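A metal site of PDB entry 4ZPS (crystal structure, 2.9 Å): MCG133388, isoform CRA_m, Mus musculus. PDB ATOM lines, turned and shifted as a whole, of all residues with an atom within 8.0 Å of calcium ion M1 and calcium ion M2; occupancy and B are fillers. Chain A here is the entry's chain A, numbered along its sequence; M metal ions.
OE2 of Glu 8 binds calcium ion M2, 2.4 Å away. Calcium ion M2 is bound by OD2 of Asp 96 (2.4 Å). OE2 of Glu 64 is bound to calcium ion M2, 2.5 Å away. Calcium ion M2 is bound by the backbone carbonyl oxygen (O) of Ile 97 (2.6 Å). Calcium ion M2 has four donor atoms within binding distance. Slightly farther from calcium ion M2 lies the side-chain carboxylate (OD1) of Asp 132 (3.1 Å).
Four residues have an atom within 4 Å of calcium ion M1: Glu 8, Asp 62, Glu 64 and Asp 99.
The backbone NH of Arg 63 sits at hydrogen-bond distance from the side-chain carboxylate of Glu 8. N of Glu 8 lies within hydrogen-bond range of O of Thr 95. OD2 of Asp 96 lies close to NE of Arg 63 (3.7 Å). The side-chain carboxylate (OD2) of Asp 62 is in salt-bridge range of the guanidinium group (NH2) of Arg 60 (3.0 Å).
Calcium ion M1 is bound by OD2 of Asp 99 (2.4 Å). The side-chain carboxylate (OD1) of Asp 62 binds calcium ion M1 (2.4 Å). Calcium ion M1 is bound by OE1 of Glu 64 (2.5 Å). The side-chain carboxylate (OE2) of Glu 8 binds calcium ion M1. The side-chain carboxylate (OD1) of Asp 99 is bound to calcium ion M1 (2.5 Å). Calcium ion M1 has five donor atoms within binding distance. Slightly farther from calcium ion M1 lies OE1 of Glu 8 (3.0 Å).
Six residues have an atom within 4 Å of calcium ion M2: Glu 8, Glu 64, Asp 96, Ile 97, Asp 99 and Asp 132.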
ATOM      1  N   PRO A   7     -18.165  15.837  22.947  1.00  0.00           N
ATOM      2  CA  PRO A   7     -17.017  15.260  22.254  1.00  0.00           C
ATOM      3  C   PRO A   7     -16.894  15.761  20.814  1.00  0.00           C
ATOM      4  O   PRO A   7     -17.891  16.146  20.210  1.00  0.00           O
ATOM      5  CB  PRO A   7     -17.307  13.757  22.279  1.00  0.00           C
ATOM      6  CG  PRO A   7     -18.186  13.567  23.462  1.00  0.00           C
ATOM      7  CD  PRO A   7     -19.039  14.791  23.520  1.00  0.00           C
ATOM      8  N   GLU A   8     -15.667  15.758  20.287  1.00  0.00           N
ATOM      9  CA  GLU A   8     -15.430  16.191  18.921  1.00  0.00           C
ATOM     10  C   GLU A   8     -15.724  15.079  17.923  1.00  0.00           C
ATOM     11  O   GLU A   8     -16.009  13.952  18.319  1.00  0.00           O
ATOM     12  CB  GLU A   8     -13.976  16.662  18.757  1.00  0.00           C
ATOM     13  CG  GLU A   8     -12.961  15.552  18.913  1.00  0.00           C
ATOM     14  CD  GLU A   8     -11.537  16.036  18.752  1.00  0.00           C
ATOM     15  OE1 GLU A   8     -11.336  17.252  18.543  1.00  0.00           O
ATOM     16  OE2 GLU A   8     -10.609  15.207  18.833  1.00  0.00           O
ATOM     17  N   GLU A   9     -15.655  15.414  16.632  1.00  0.00           N
ATOM     18  CA  GLU A   9     -15.853  14.452  15.547  1.00  0.00           C
ATOM     19  C   GLU A   9     -17.155  13.673  15.666  1.00  0.00           C
ATOM     20  O   GLU A   9     -17.282  12.574  15.137  1.00  0.00           O
ATOM     21  CB  GLU A   9     -14.671  13.482  15.470  1.00  0.00           C
ATOM     22  N   THR A  10     -18.127  14.256  16.373  1.00  0.00           N
ATOM     23  CA  THR A  10     -19.406  13.597  16.597  1.00  0.00           C
ATOM     24  C   THR A  10     -20.336  13.795  15.406  1.00  0.00           C
ATOM     25  O   THR A  10     -20.043  14.580  14.511  1.00  0.00           O
ATOM     26  CB  THR A  10     -20.090  14.124  17.878  1.00  0.00           C
ATOM     27  OG1 THR A  10     -21.305  13.408  18.109  1.00  0.00           O
ATOM     28  CG2 THR A  10     -20.394  15.606  17.754  1.00  0.00           C
ATOM     29  N   ARG A  60     -20.175  19.143  11.423  1.00  0.00           N
ATOM     30  CA  ARG A  60     -18.926  18.535  11.869  1.00  0.00           C
ATOM     31  C   ARG A  60     -18.234  19.396  12.926  1.00  0.00           C
ATOM     32  O   ARG A  60     -18.112  20.604  12.760  1.00  0.00           O
ATOM     33  CB  ARG A  60     -17.977  18.325  10.684  1.00  0.00           C
ATOM     34  CG  ARG A  60     -16.656  17.679  11.070  1.00  0.00           C
ATOM     35  CD  ARG A  60     -15.492  18.237  10.263  1.00  0.00           C
ATOM     36  NE  ARG A  60     -14.210  17.786  10.781  1.00  0.00           N
ATOM     37  CZ  ARG A  60     -13.034  18.215  10.345  1.00  0.00           C
ATOM     38  NH1 ARG A  60     -12.963  19.121   9.386  1.00  0.00           N
ATOM     39  NH2 ARG A  60     -11.920  17.735  10.882  1.00  0.00           N
ATOM     40  N   ILE A  61     -17.804  18.759  14.008  1.00  0.00           N
ATOM     41  CA  ILE A  61     -17.121  19.473  15.087  1.00  0.00           C
ATOM     42  C   ILE A  61     -15.751  18.855  15.365  1.00  0.00           C
ATOM     43  O   ILE A  61     -15.648  17.712  15.803  1.00  0.00           O
ATOM     44  CB  ILE A  61     -17.949  19.447  16.389  1.00  0.00           C
ATOM     45  CG1 ILE A  61     -19.328  20.066  16.156  1.00  0.00           C
ATOM     46  CG2 ILE A  61     -17.220  20.184  17.501  1.00  0.00           C
ATOM     47  CD1 ILE A  61     -20.182  20.143  17.394  1.00  0.00           C
ATOM     48  N   ASP A  62     -14.700  19.629  15.111  1.00  0.00           N
ATOM     49  CA  ASP A  62     -13.346  19.178  15.376  1.00  0.00           C
ATOM     50  C   ASP A  62     -12.516  20.279  16.032  1.00  0.00           C
ATOM     51  O   ASP A  62     -12.425  21.392  15.498  1.00  0.00           O
ATOM     52  CB  ASP A  62     -12.669  18.698  14.088  1.00  0.00           C
ATOM     53  CG  ASP A  62     -11.874  17.416  14.292  1.00  0.00           C
ATOM     54  OD1 ASP A  62     -12.313  16.573  15.099  1.00  0.00           O
ATOM     55  OD2 ASP A  62     -10.828  17.256  13.638  1.00  0.00           O
ATOM     56  N   ARG A  63     -11.913  19.971  17.175  1.00  0.00           N
ATOM     57  CA  ARG A  63     -11.140  20.941  17.946  1.00  0.00           C
ATOM     58  C   ARG A  63      -9.912  21.439  17.187  1.00  0.00           C
ATOM     59  O   ARG A  63      -9.499  22.588  17.332  1.00  0.00           O
ATOM     60  CB  ARG A  63     -10.721  20.318  19.288  1.00  0.00           C
ATOM     61  CG  ARG A  63      -9.672  21.103  20.055  1.00  0.00           C
ATOM     62  CD  ARG A  63      -9.439  20.523  21.434  1.00  0.00           C
ATOM     63  NE  ARG A  63      -8.142  20.917  21.986  1.00  0.00           N
ATOM     64  CZ  ARG A  63      -7.743  20.667  23.226  1.00  0.00           C
ATOM     65  NH1 ARG A  63      -8.555  20.030  24.069  1.00  0.00           N
ATOM     66  NH2 ARG A  63      -6.548  21.055  23.638  1.00  0.00           N
ATOM     67  N   GLU A  64      -9.338  20.566  16.354  1.00  0.00           N
ATOM     68  CA  GLU A  64      -8.122  20.894  15.608  1.00  0.00           C
ATOM     69  C   GLU A  64      -8.316  22.100  14.683  1.00  0.00           C
ATOM     70  O   GLU A  64      -7.402  22.909  14.509  1.00  0.00           O
ATOM     71  CB  GLU A  64      -7.658  19.683  14.784  1.00  0.00           C
ATOM     72  CG  GLU A  64      -7.018  18.580  15.607  1.00  0.00           C
ATOM     73  CD  GLU A  64      -8.010  17.844  16.485  1.00  0.00           C
ATOM     74  OE1 GLU A  64      -8.775  17.015  15.945  1.00  0.00           O
ATOM     75  OE2 GLU A  64      -8.024  18.095  17.709  1.00  0.00           O
ATOM     76  N   GLU A  65      -9.506  22.220  14.102  1.00  0.00           N
ATOM     77  CA  GLU A  65      -9.806  23.318  13.192  1.00  0.00           C
ATOM     78  C   GLU A  65     -10.485  24.454  13.934  1.00  0.00           C
ATOM     79  O   GLU A  65     -10.514  25.593  13.454  1.00  0.00           O
ATOM     80  CB  GLU A  65     -10.669  22.830  12.035  1.00  0.00           C
ATOM     81  CG  GLU A  65     -10.811  23.825  10.887  1.00  0.00           C
ATOM     82  CD  GLU A  65     -11.615  23.275   9.731  1.00  0.00           C
ATOM     83  OE1 GLU A  65     -11.971  22.086   9.769  1.00  0.00           O
ATOM     84  OE2 GLU A  65     -11.897  24.044   8.783  1.00  0.00           O
ATOM     85  N   ALA A  68      -7.615  23.881  18.328  1.00  0.00           N
ATOM     86  CA  ALA A  68      -6.270  23.349  18.166  1.00  0.00           C
ATOM     87  C   ALA A  68      -5.424  23.471  19.423  1.00  0.00           C
ATOM     88  O   ALA A  68      -5.567  22.676  20.362  1.00  0.00           O
ATOM     89  CB  ALA A  68      -5.567  24.029  16.989  1.00  0.00           C
ATOM     90  N   ILE A  94     -15.644  21.504  24.321  1.00  0.00           N
ATOM     91  CA  ILE A  94     -15.447  20.452  23.330  1.00  0.00           C
ATOM     92  C   ILE A  94     -14.334  19.489  23.756  1.00  0.00           C
ATOM     93  O   ILE A  94     -13.186  19.909  23.963  1.00  0.00           O
ATOM     94  CB  ILE A  94     -15.121  21.022  21.937  1.00  0.00           C
ATOM     95  CG1 ILE A  94     -16.284  21.896  21.439  1.00  0.00           C
ATOM     96  CG2 ILE A  94     -14.829  19.900  20.950  1.00  0.00           C
ATOM     97  CD1 ILE A  94     -16.048  22.491  20.067  1.00  0.00           C
ATOM     98  N   THR A  95     -14.673  18.211  23.873  1.00  0.00           N
ATOM     99  CA  THR A  95     -13.703  17.201  24.310  1.00  0.00           C
ATOM    100  C   THR A  95     -12.765  16.809  23.169  1.00  0.00           C
ATOM    101  O   THR A  95     -13.207  16.516  22.066  1.00  0.00           O
ATOM    102  CB  THR A  95     -14.416  15.937  24.842  1.00  0.00           C
ATOM    103  OG1 THR A  95     -15.248  16.290  25.960  1.00  0.00           O
ATOM    104  CG2 THR A  95     -13.407  14.896  25.286  1.00  0.00           C
ATOM    105  N   ASP A  96     -11.462  16.821  23.457  1.00  0.00           N
ATOM    106  CA  ASP A  96     -10.455  16.406  22.487  1.00  0.00           C
ATOM    107  C   ASP A  96     -10.334  14.895  22.442  1.00  0.00           C
ATOM    108  O   ASP A  96     -10.271  14.235  23.484  1.00  0.00           O
ATOM    109  CB  ASP A  96      -9.092  17.040  22.832  1.00  0.00           C
ATOM    110  CG  ASP A  96      -7.992  16.619  21.874  1.00  0.00           C
ATOM    111  OD1 ASP A  96      -7.378  15.552  22.089  1.00  0.00           O
ATOM    112  OD2 ASP A  96      -7.720  17.366  20.914  1.00  0.00           O
ATOM    113  N   ILE A  97     -10.315  14.344  21.238  1.00  0.00           N
ATOM    114  CA  ILE A  97     -10.120  12.907  21.046  1.00  0.00           C
ATOM    115  C   ILE A  97      -8.844  12.664  20.253  1.00  0.00           C
ATOM    116  O   ILE A  97      -8.295  13.586  19.645  1.00  0.00           O
ATOM    117  CB  ILE A  97     -11.312  12.263  20.326  1.00  0.00           C
ATOM    118  N   ASN A  98      -8.369  11.420  20.259  1.00  0.00           N
ATOM    119  CA  ASN A  98      -7.145  11.071  19.548  1.00  0.00           C
ATOM    120  C   ASN A  98      -7.417  10.621  18.121  1.00  0.00           C
ATOM    121  O   ASN A  98      -7.709   9.456  17.873  1.00  0.00           O
ATOM    122  CB  ASN A  98      -6.390   9.981  20.301  1.00  0.00           C
ATOM    123  CG  ASN A  98      -4.925   9.922  19.936  1.00  0.00           C
ATOM    124  OD1 ASN A  98      -4.515  10.415  18.886  1.00  0.00           O
ATOM    125  ND2 ASN A  98      -4.114   9.324  20.800  1.00  0.00           N
ATOM    126  N   ASP A  99      -7.339  11.566  17.185  1.00  0.00           N
ATOM    127  CA  ASP A  99      -7.538  11.257  15.764  1.00  0.00           C
ATOM    128  C   ASP A  99      -6.448  11.894  14.919  1.00  0.00           C
ATOM    129  O   ASP A  99      -6.527  11.904  13.685  1.00  0.00           O
ATOM    130  CB  ASP A  99      -8.917  11.724  15.303  1.00  0.00           C
ATOM    131  CG  ASP A  99      -9.112  13.223  15.486  1.00  0.00           C
ATOM    132  OD1 ASP A  99      -8.618  13.781  16.483  1.00  0.00           O
ATOM    133  OD2 ASP A  99      -9.754  13.842  14.610  1.00  0.00           O
ATOM    134  N   ASN A 100      -5.434  12.443  15.590  1.00  0.00           N
ATOM    135  CA  ASN A 100      -4.330  13.101  14.894  1.00  0.00           C
ATOM    136  C   ASN A 100      -2.985  12.820  15.566  1.00  0.00           C
ATOM    137  O   ASN A 100      -2.541  13.562  16.440  1.00  0.00           O
ATOM    138  CB  ASN A 100      -4.582  14.608  14.833  1.00  0.00           C
ATOM    139  N   PRO A 131      -1.321  17.810  16.378  1.00  0.00           N
ATOM    140  CA  PRO A 131      -2.527  18.636  16.282  1.00  0.00           C
ATOM    141  C   PRO A 131      -3.329  18.628  17.572  1.00  0.00           C
ATOM    142  O   PRO A 131      -3.840  19.671  17.997  1.00  0.00           O
ATOM    143  CB  PRO A 131      -3.310  17.986  15.136  1.00  0.00           C
ATOM    144  CG  PRO A 131      -2.265  17.312  14.312  1.00  0.00           C
ATOM    145  CD  PRO A 131      -1.243  16.811  15.297  1.00  0.00           C
ATOM    146  N   ASP A 132      -3.443  17.459  18.194  1.00  0.00           N
ATOM    147  CA  ASP A 132      -4.099  17.329  19.485  1.00  0.00           C
ATOM    148  C   ASP A 132      -3.144  17.780  20.594  1.00  0.00           C
ATOM    149  O   ASP A 132      -1.927  17.701  20.423  1.00  0.00           O
ATOM    150  CB  ASP A 132      -4.564  15.902  19.722  1.00  0.00           C
ATOM    151  CG  ASP A 132      -5.061  15.227  18.462  1.00  0.00           C
ATOM    152  OD1 ASP A 132      -5.609  15.938  17.584  1.00  0.00           O
ATOM    153  OD2 ASP A 132      -4.899  14.004  18.335  1.00  0.00           O
ATOM    154  N   VAL A 133      -3.698  18.240  21.705  1.00  0.00           N
ATOM    155  CA  VAL A 133      -2.874  18.707  22.817  1.00  0.00           C
ATOM    156  C   VAL A 133      -3.252  17.976  24.107  1.00  0.00           C
ATOM    157  O   VAL A 133      -4.436  17.696  24.351  1.00  0.00           O
ATOM    158  CB  VAL A 133      -3.024  20.229  23.034  1.00  0.00           C
ATOM    159  CG1 VAL A 133      -2.029  20.724  24.068  1.00  0.00           C
ATOM    160  CG2 VAL A 133      -2.832  20.972  21.719  1.00  0.00           C
ATOM    161  N   ASN A 136      -3.072  13.256  24.422  1.00  0.00           N
ATOM    162  CA  ASN A 136      -3.221  12.890  23.024  1.00  0.00           C
ATOM    163  C   ASN A 136      -2.311  13.702  22.119  1.00  0.00           C
ATOM    164  O   ASN A 136      -2.567  13.845  20.926  1.00  0.00           O
ATOM    165  CB  ASN A 136      -4.678  13.046  22.581  1.00  0.00           C
ATOM    166  CG  ASN A 136      -5.633  12.254  23.439  1.00  0.00           C
ATOM    167  OD1 ASN A 136      -5.794  11.051  23.268  1.00  0.00           O
ATOM    168  ND2 ASN A 136      -6.291  12.942  24.364  1.00  0.00           N
HETATM  169 CA    CA M   1     -10.566  15.378  16.326  1.00  0.00          CA
HETATM  170 CA    CA M   2      -8.406  16.059  19.023  1.00  0.00          CA
HETATM  171 CA    CA M   3      -2.680  12.154  18.475  1.00  0.00          CA
